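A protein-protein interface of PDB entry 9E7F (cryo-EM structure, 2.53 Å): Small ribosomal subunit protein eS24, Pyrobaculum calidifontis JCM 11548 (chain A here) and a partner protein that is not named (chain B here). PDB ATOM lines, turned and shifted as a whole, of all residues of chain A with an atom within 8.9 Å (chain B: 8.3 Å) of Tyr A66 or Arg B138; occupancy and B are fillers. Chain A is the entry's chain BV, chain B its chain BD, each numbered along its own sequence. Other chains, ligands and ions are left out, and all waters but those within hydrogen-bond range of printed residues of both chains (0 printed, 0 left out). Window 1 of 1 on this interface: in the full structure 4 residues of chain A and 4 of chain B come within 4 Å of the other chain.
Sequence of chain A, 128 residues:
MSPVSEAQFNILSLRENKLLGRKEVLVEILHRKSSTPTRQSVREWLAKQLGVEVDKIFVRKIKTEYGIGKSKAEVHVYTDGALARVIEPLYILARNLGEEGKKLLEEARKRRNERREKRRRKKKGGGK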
ATOM      1  N   LYS A  63      -9.597  -7.691   5.744  1.00  0.00           N
ATOM      2  CA  LYS A  63      -8.485  -7.416   6.646  1.00  0.00           C
ATOM      3  C   LYS A  63      -7.234  -7.168   5.817  1.00  0.00           C
ATOM      4  O   LYS A  63      -6.872  -7.994   4.971  1.00  0.00           O
ATOM      5  CB  LYS A  63      -8.278  -8.577   7.619  1.00  0.00           C
ATOM      6  CG  LYS A  63      -6.833  -9.018   7.799  1.00  0.00           C
ATOM      7  CD  LYS A  63      -6.317  -8.715   9.202  1.00  0.00           C
ATOM      8  CE  LYS A  63      -5.049  -9.505   9.503  1.00  0.00           C
ATOM      9  NZ  LYS A  63      -4.295  -8.969  10.670  1.00  0.00           N
ATOM     10  N   THR A  64      -6.579  -6.038   6.058  1.00  0.00           N
ATOM     11  CA  THR A  64      -5.440  -5.605   5.262  1.00  0.00           C
ATOM     12  C   THR A  64      -4.150  -5.810   6.041  1.00  0.00           C
ATOM     13  O   THR A  64      -4.053  -5.411   7.204  1.00  0.00           O
ATOM     14  CB  THR A  64      -5.577  -4.138   4.866  1.00  0.00           C
ATOM     15  OG1 THR A  64      -6.933  -3.872   4.494  1.00  0.00           O
ATOM     16  CG2 THR A  64      -4.666  -3.821   3.697  1.00  0.00           C
ATOM     17  N   GLU A  65      -3.163  -6.413   5.391  1.00  0.00           N
ATOM     18  CA  GLU A  65      -1.896  -6.703   6.038  1.00  0.00           C
ATOM     19  C   GLU A  65      -1.131  -5.416   6.327  1.00  0.00           C
ATOM     20  O   GLU A  65      -1.379  -4.362   5.739  1.00  0.00           O
ATOM     21  CB  GLU A  65      -1.052  -7.625   5.161  1.00  0.00           C
ATOM     22  CG  GLU A  65      -1.864  -8.655   4.401  1.00  0.00           C
ATOM     23  CD  GLU A  65      -1.129  -9.966   4.215  1.00  0.00           C
ATOM     24  OE1 GLU A  65       0.106  -9.938   4.035  1.00  0.00           O
ATOM     25  OE2 GLU A  65      -1.788 -11.025   4.243  1.00  0.00           O
ATOM     26  N   TYR A  66      -0.186  -5.518   7.253  1.00  0.00           N
ATOM     27  CA  TYR A  66       0.666  -4.388   7.586  1.00  0.00           C
ATOM     28  C   TYR A  66       1.703  -4.154   6.492  1.00  0.00           C
ATOM     29  O   TYR A  66       2.254  -5.098   5.923  1.00  0.00           O
ATOM     30  CB  TYR A  66       1.362  -4.643   8.923  1.00  0.00           C
ATOM     31  CG  TYR A  66       2.119  -3.465   9.483  1.00  0.00           C
ATOM     32  CD1 TYR A  66       1.489  -2.534  10.290  1.00  0.00           C
ATOM     33  CD2 TYR A  66       3.467  -3.287   9.211  1.00  0.00           C
ATOM     34  CE1 TYR A  66       2.175  -1.461  10.805  1.00  0.00           C
ATOM     35  CE2 TYR A  66       4.160  -2.212   9.717  1.00  0.00           C
ATOM     36  CZ  TYR A  66       3.509  -1.305  10.516  1.00  0.00           C
ATOM     37  OH  TYR A  66       4.198  -0.236  11.025  1.00  0.00           O
ATOM     38  N   GLY A  67       1.958  -2.885   6.191  1.00  0.00           N
ATOM     39  CA  GLY A  67       3.119  -2.513   5.410  1.00  0.00           C
ATOM     40  C   GLY A  67       3.063  -2.794   3.927  1.00  0.00           C
ATOM     41  O   GLY A  67       4.092  -2.667   3.256  1.00  0.00           O
ATOM     42  N   ILE A  68       1.908  -3.172   3.386  1.00  0.00           N
ATOM     43  CA  ILE A  68       1.786  -3.468   1.963  1.00  0.00           C
ATOM     44  C   ILE A  68       0.308  -3.489   1.618  1.00  0.00           C
ATOM     45  O   ILE A  68      -0.538  -3.778   2.464  1.00  0.00           O
ATOM     46  CB  ILE A  68       2.473  -4.811   1.608  1.00  0.00           C
ATOM     47  CG1 ILE A  68       2.523  -5.008   0.093  1.00  0.00           C
ATOM     48  CG2 ILE A  68       1.759  -5.971   2.279  1.00  0.00           C
ATOM     49  CD1 ILE A  68       3.487  -6.066  -0.355  1.00  0.00           C
ATOM     50  N   GLY A  69      -0.009  -3.183   0.365  1.00  0.00           N
ATOM     51  CA  GLY A  69      -1.380  -3.216  -0.092  1.00  0.00           C
ATOM     52  C   GLY A  69      -1.853  -4.615  -0.427  1.00  0.00           C
ATOM     53  O   GLY A  69      -1.948  -4.984  -1.599  1.00  0.00           O
ATOM     54  N   LYS A  70      -2.138  -5.410   0.602  1.00  0.00           N
ATOM     55  CA  LYS A  70      -2.677  -6.750   0.435  1.00  0.00           C
ATOM     56  C   LYS A  70      -3.790  -6.970   1.444  1.00  0.00           C
ATOM     57  O   LYS A  70      -3.667  -6.572   2.606  1.00  0.00           O
ATOM     58  CB  LYS A  70      -1.595  -7.810   0.615  1.00  0.00           C
ATOM     59  CG  LYS A  70      -1.545  -8.823  -0.493  1.00  0.00           C
ATOM     60  CD  LYS A  70      -0.738 -10.032  -0.087  1.00  0.00           C
ATOM     61  CE  LYS A  70       0.701  -9.655   0.189  1.00  0.00           C
ATOM     62  NZ  LYS A  70       1.624 -10.808   0.007  1.00  0.00           N
ATOM     63  N   SER A  71      -4.869  -7.611   1.006  1.00  0.00           N
ATOM     64  CA  SER A  71      -6.021  -7.836   1.865  1.00  0.00           C
ATOM     65  C   SER A  71      -6.526  -9.258   1.696  1.00  0.00           C
ATOM     66  O   SER A  71      -6.294  -9.910   0.678  1.00  0.00           O
ATOM     67  CB  SER A  71      -7.155  -6.850   1.569  1.00  0.00           C
ATOM     68  OG  SER A  71      -6.651  -5.567   1.260  1.00  0.00           O
ATOM     69  N   LYS A  72      -7.218  -9.734   2.725  1.00  0.00           N
ATOM     70  CA  LYS A  72      -7.935 -10.998   2.685  1.00  0.00           C
ATOM     71  C   LYS A  72      -9.367 -10.746   3.121  1.00  0.00           C
ATOM     72  O   LYS A  72      -9.603 -10.074   4.129  1.00  0.00           O
ATOM     73  CB  LYS A  72      -7.280 -12.041   3.586  1.00  0.00           C
ATOM     74  CG  LYS A  72      -7.288 -13.431   3.002  1.00  0.00           C
ATOM     75  CD  LYS A  72      -5.938 -14.096   3.146  1.00  0.00           C
ATOM     76  CE  LYS A  72      -5.388 -13.911   4.545  1.00  0.00           C
ATOM     77  NZ  LYS A  72      -4.033 -14.499   4.679  1.00  0.00           N
ATOM     78  N   LEU B 108      17.850  -4.871  12.242  1.00  0.00           N
ATOM     79  CA  LEU B 108      17.493  -4.461  10.888  1.00  0.00           C
ATOM     80  C   LEU B 108      18.155  -3.144  10.517  1.00  0.00           C
ATOM     81  O   LEU B 108      18.496  -2.921   9.353  1.00  0.00           O
ATOM     82  CB  LEU B 108      15.977  -4.348  10.755  1.00  0.00           C
ATOM     83  CG  LEU B 108      15.472  -3.788   9.427  1.00  0.00           C
ATOM     84  CD1 LEU B 108      16.109  -4.519   8.266  1.00  0.00           C
ATOM     85  CD2 LEU B 108      13.962  -3.886   9.353  1.00  0.00           C
ATOM     86  N   VAL B 128      14.356   3.000   8.030  1.00  0.00           N
ATOM     87  CA  VAL B 128      13.417   2.007   8.533  1.00  0.00           C
ATOM     88  C   VAL B 128      12.240   2.687   9.213  1.00  0.00           C
ATOM     89  O   VAL B 128      11.096   2.234   9.110  1.00  0.00           O
ATOM     90  CB  VAL B 128      14.142   1.042   9.483  1.00  0.00           C
ATOM     91  CG1 VAL B 128      13.198  -0.030   9.975  1.00  0.00           C
ATOM     92  CG2 VAL B 128      15.334   0.429   8.785  1.00  0.00           C
ATOM     93  N   VAL B 129      12.507   3.783   9.920  1.00  0.00           N
ATOM     94  CA  VAL B 129      11.465   4.457  10.688  1.00  0.00           C
ATOM     95  C   VAL B 129      10.424   5.076   9.767  1.00  0.00           C
ATOM     96  O   VAL B 129       9.220   5.006  10.034  1.00  0.00           O
ATOM     97  CB  VAL B 129      12.094   5.507  11.617  1.00  0.00           C
ATOM     98  CG1 VAL B 129      11.060   6.531  12.012  1.00  0.00           C
ATOM     99  CG2 VAL B 129      12.673   4.832  12.840  1.00  0.00           C
ATOM    100  N   GLY B 131       9.739   4.078   6.775  1.00  0.00           N
ATOM    101  CA  GLY B 131       9.075   3.061   5.990  1.00  0.00           C
ATOM    102  C   GLY B 131       9.556   2.975   4.559  1.00  0.00           C
ATOM    103  O   GLY B 131       8.747   2.930   3.630  1.00  0.00           O
ATOM    104  N   HIS B 132      10.869   2.963   4.361  1.00  0.00           N
ATOM    105  CA  HIS B 132      11.442   2.787   3.037  1.00  0.00           C
ATOM    106  C   HIS B 132      12.181   1.470   2.892  1.00  0.00           C
ATOM    107  O   HIS B 132      12.819   1.240   1.862  1.00  0.00           O
ATOM    108  CB  HIS B 132      12.378   3.943   2.704  1.00  0.00           C
ATOM    109  CG  HIS B 132      11.781   5.287   2.957  1.00  0.00           C
ATOM    110  ND1 HIS B 132      10.538   5.645   2.487  1.00  0.00           N
ATOM    111  CD2 HIS B 132      12.265   6.369   3.609  1.00  0.00           C
ATOM    112  CE1 HIS B 132      10.275   6.886   2.853  1.00  0.00           C
ATOM    113  NE2 HIS B 132      11.307   7.349   3.532  1.00  0.00           N
ATOM    114  N   VAL B 133      12.105   0.598   3.888  1.00  0.00           N
ATOM    115  CA  VAL B 133      12.834  -0.660   3.880  1.00  0.00           C
ATOM    116  C   VAL B 133      11.825  -1.793   3.796  1.00  0.00           C
ATOM    117  O   VAL B 133      11.053  -2.018   4.735  1.00  0.00           O
ATOM    118  CB  VAL B 133      13.722  -0.800   5.122  1.00  0.00           C
ATOM    119  CG1 VAL B 133      14.441  -2.128   5.101  1.00  0.00           C
ATOM    120  CG2 VAL B 133      14.706   0.349   5.178  1.00  0.00           C
ATOM    121  N   LEU B 134      11.846  -2.514   2.683  1.00  0.00           N
ATOM    122  CA  LEU B 134      10.924  -3.611   2.444  1.00  0.00           C
ATOM    123  C   LEU B 134      11.649  -4.921   2.705  1.00  0.00           C
ATOM    124  O   LEU B 134      12.716  -5.168   2.137  1.00  0.00           O
ATOM    125  CB  LEU B 134      10.391  -3.588   1.010  1.00  0.00           C
ATOM    126  CG  LEU B 134       9.291  -2.610   0.578  1.00  0.00           C
ATOM    127  CD1 LEU B 134       7.939  -3.017   1.123  1.00  0.00           C
ATOM    128  CD2 LEU B 134       9.603  -1.166   0.932  1.00  0.00           C
ATOM    129  N   VAL B 135      11.079  -5.751   3.567  1.00  0.00           N
ATOM    130  CA  VAL B 135      11.633  -7.060   3.876  1.00  0.00           C
ATOM    131  C   VAL B 135      10.743  -8.085   3.187  1.00  0.00           C
ATOM    132  O   VAL B 135       9.629  -8.364   3.640  1.00  0.00           O
ATOM    133  CB  VAL B 135      11.719  -7.308   5.384  1.00  0.00           C
ATOM    134  CG1 VAL B 135      12.126  -8.741   5.656  1.00  0.00           C
ATOM    135  CG2 VAL B 135      12.699  -6.343   6.016  1.00  0.00           C
ATOM    136  N   ALA B 136      11.235  -8.647   2.085  1.00  0.00           N
ATOM    137  CA  ALA B 136      10.487  -9.572   1.245  1.00  0.00           C
ATOM    138  C   ALA B 136       9.228  -8.947   0.669  1.00  0.00           C
ATOM    139  O   ALA B 136       8.243  -9.646   0.429  1.00  0.00           O
ATOM    140  CB  ALA B 136      10.132 -10.853   2.003  1.00  0.00           C
ATOM    141  N   GLY B 137       9.239  -7.640   0.432  1.00  0.00           N
ATOM    142  CA  GLY B 137       8.113  -6.947  -0.154  1.00  0.00           C
ATOM    143  C   GLY B 137       7.221  -6.246   0.838  1.00  0.00           C
ATOM    144  O   GLY B 137       6.341  -5.486   0.420  1.00  0.00           O
ATOM    145  N   ARG B 138       7.418  -6.462   2.133  1.00  0.00           N
ATOM    146  CA  ARG B 138       6.606  -5.837   3.164  1.00  0.00           C
ATOM    147  C   ARG B 138       7.427  -4.803   3.918  1.00  0.00           C
ATOM    148  O   ARG B 138       8.621  -4.999   4.162  1.00  0.00           O
ATOM    149  CB  ARG B 138       6.052  -6.882   4.136  1.00  0.00           C
ATOM    150  CG  ARG B 138       5.194  -6.301   5.239  1.00  0.00           C
ATOM    151  CD  ARG B 138       4.895  -7.333   6.300  1.00  0.00           C
ATOM    152  NE  ARG B 138       4.433  -8.587   5.720  1.00  0.00           N
ATOM    153  CZ  ARG B 138       3.180  -8.821   5.358  1.00  0.00           C
ATOM    154  NH1 ARG B 138       2.232  -7.917   5.532  1.00  0.00           N
ATOM    155  NH2 ARG B 138       2.870  -9.991   4.810  1.00  0.00           N
ATOM    156  N   ARG B 139       6.781  -3.702   4.278  1.00  0.00           N
ATOM    157  CA  ARG B 139       7.428  -2.639   5.031  1.00  0.00           C
ATOM    158  C   ARG B 139       7.599  -3.060   6.482  1.00  0.00           C
ATOM    159  O   ARG B 139       6.616  -3.346   7.172  1.00  0.00           O
ATOM    160  CB  ARG B 139       6.603  -1.362   4.940  1.00  0.00           C
ATOM    161  CG  ARG B 139       7.172  -0.336   4.012  1.00  0.00           C
ATOM    162  CD  ARG B 139       6.483   0.980   4.218  1.00  0.00           C
ATOM    163  NE  ARG B 139       5.195   1.003   3.542  1.00  0.00           N
ATOM    164  CZ  ARG B 139       4.028   0.817   4.144  1.00  0.00           C
ATOM    165  NH1 ARG B 139       3.950   0.584   5.442  1.00  0.00           N
ATOM    166  NH2 ARG B 139       2.913   0.870   3.424  1.00  0.00           N
ATOM    167  N   VAL B 140       8.839  -3.096   6.945  1.00  0.00           N
ATOM    168  CA  VAL B 140       9.157  -3.425   8.327  1.00  0.00           C
ATOM    169  C   VAL B 140       9.805  -2.187   8.928  1.00  0.00           C
ATOM    170  O   VAL B 140      10.956  -1.865   8.620  1.00  0.00           O
ATOM    171  CB  VAL B 140      10.073  -4.647   8.428  1.00  0.00           C
ATOM    172  CG1 VAL B 140      10.739  -4.689   9.784  1.00  0.00           C
ATOM    173  CG2 VAL B 140       9.288  -5.918   8.170  1.00  0.00           C
ATOM    174  N   THR B 141       9.075  -1.491   9.794  1.00  0.00           N
ATOM    175  CA  THR B 141       9.474  -0.173  10.263  1.00  0.00           C
ATOM    176  C   THR B 141      10.121  -0.186  11.643  1.00  0.00           C
ATOM    177  O   THR B 141      10.360   0.884  12.208  1.00  0.00           O
ATOM    178  CB  THR B 141       8.266   0.763  10.262  1.00  0.00           C
ATOM    179  OG1 THR B 141       7.215   0.181  11.035  1.00  0.00           O
ATOM    180  CG2 THR B 141       7.768   0.978   8.847  1.00  0.00           C
ATOM    181  N   SER B 142      10.421  -1.357  12.198  1.00  0.00           N
ATOM    182  CA  SER B 142      11.035  -1.417  13.514  1.00  0.00           C
ATOM    183  C   SER B 142      12.535  -1.588  13.359  1.00  0.00           C
ATOM    184  O   SER B 142      12.981  -2.667  12.943  1.00  0.00           O
ATOM    185  CB  SER B 142      10.450  -2.566  14.329  1.00  0.00           C
ATOM    186  OG  SER B 142      10.590  -2.324  15.716  1.00  0.00           O
ATOM    187  N   PHE B 145      14.492  -4.730  14.645  1.00  0.00           N
ATOM    188  CA  PHE B 145      14.090  -6.045  14.169  1.00  0.00           C
ATOM    189  C   PHE B 145      15.310  -6.939  13.986  1.00  0.00           C
ATOM    190  O   PHE B 145      16.261  -6.575  13.289  1.00  0.00           O
ATOM    191  CB  PHE B 145      13.322  -5.886  12.858  1.00  0.00           C
ATOM    192  CG  PHE B 145      13.014  -7.177  12.164  1.00  0.00           C
ATOM    193  CD1 PHE B 145      12.450  -8.236  12.845  1.00  0.00           C
ATOM    194  CD2 PHE B 145      13.272  -7.321  10.816  1.00  0.00           C
ATOM    195  CE1 PHE B 145      12.167  -9.416  12.197  1.00  0.00           C
ATOM    196  CE2 PHE B 145      12.990  -8.496  10.166  1.00  0.00           C
ATOM    197  CZ  PHE B 145      12.437  -9.544  10.856  1.00  0.00           C
ATOM    198  N   LYS B 154      16.536 -10.508   1.273  1.00  0.00           N
ATOM    199  CA  LYS B 154      15.323  -9.921   0.724  1.00  0.00           C
ATOM    200  C   LYS B 154      15.173  -8.444   1.061  1.00  0.00           C
ATOM    201  O   LYS B 154      14.166  -7.831   0.695  1.00  0.00           O
ATOM    202  CB  LYS B 154      14.097 -10.688   1.216  1.00  0.00           C
ATOM    203  CG  LYS B 154      14.310 -12.176   1.312  1.00  0.00           C
ATOM    204  CD  LYS B 154      13.402 -12.914   0.363  1.00  0.00           C
ATOM    205  CE  LYS B 154      13.803 -14.367   0.276  1.00  0.00           C
ATOM    206  NZ  LYS B 154      15.268 -14.504   0.095  1.00  0.00           N
ATOM    207  N   ILE B 155      16.147  -7.855   1.738  1.00  0.00           N
ATOM    208  CA  ILE B 155      16.032  -6.482   2.211  1.00  0.00           C
ATOM    209  C   ILE B 155      16.242  -5.533   1.040  1.00  0.00           C
ATOM    210  O   ILE B 155      17.280  -5.574   0.371  1.00  0.00           O
ATOM    211  CB  ILE B 155      17.037  -6.203   3.337  1.00  0.00           C
ATOM    212  CG1 ILE B 155      16.537  -6.803   4.648  1.00  0.00           C
ATOM    213  CG2 ILE B 155      17.249  -4.713   3.490  1.00  0.00           C
ATOM    214  CD1 ILE B 155      17.573  -6.827   5.748  1.00  0.00           C
ATOM    215  N   THR B 156      15.252  -4.681   0.790  1.00  0.00           N
ATOM    216  CA  THR B 156      15.301  -3.715  -0.293  1.00  0.00           C
ATOM    217  C   THR B 156      14.902  -2.352   0.249  1.00  0.00           C
ATOM    218  O   THR B 156      14.450  -2.224   1.388  1.00  0.00           O
ATOM    219  CB  THR B 156      14.372  -4.102  -1.451  1.00  0.00           C
ATOM    220  OG1 THR B 156      13.072  -3.549  -1.221  1.00  0.00           O
ATOM    221  CG2 THR B 156      14.254  -5.609  -1.575  1.00  0.00           C
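NH2 of Arg B138 is in salt-bridge range of OE1 of Glu A65, 2.9 Å away.
O of Tyr A66 sits at hydrogen-bond distance from NH1 of Arg B138, 2.8 Å away.
The backbone carbonyl oxygen (O) of Gly A67 is in hydrogen-bond range of the backbone NH (N) of Arg B139 (3.1 Å).
The side-chain hydroxyl of Tyr A66 lies within hydrogen-bond range of the side-chain hydroxyl of Thr B141.
The backbone carbonyl oxygen of Lys A70 lies within hydrogen-bond range of the backbone NH of Glu A65 (2.8 Å).
Among the printed residues, merely in contact across the chains: Tyr A66 with Arg B139 (3.7 Å), Ile A68 with Gly B137 (3.0 Å) and Ile A68 with Arg B138 (3.8 Å).
Of the printed residues of chain B, Glu A65 touches Arg B138.
Of the printed residues of chain B, Tyr A66 touches Arg B138 (2.8 Å), Arg B139 (3.7 Å) and Thr B141 (3.0 Å).
Of the printed residues of chain B, Gly A67 touches Arg B139 (3.1 Å).
Of the printed residues of chain A, Gly B137 touches Ile A68 (3.0 Å).
Printed residues of chain A within 4 Å of Arg B138: Glu A65 (2.9 Å), Tyr A66 (2.8 Å) and Ile A68 (3.8 Å).
Printed residues of chain A within 4 Å of Arg B139: Tyr A66 and Gly A67.
The nearest residue of chain B that does not touch Tyr A66 is Val B140 (5.3 Å).
The nearest printed residue of chain B that does not touch Glu A65 is Arg B139 (7.2 Å).
Of the 10 printed residues of chain A, 4 touch a printed residue of chain B.
Of the 19 printed residues of chain B, 4 touch a printed residue of chain A.
Printed residues of chain B that touch a printed residue of chain A: Gly B137, Arg B138, Arg B139 and Thr B141.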
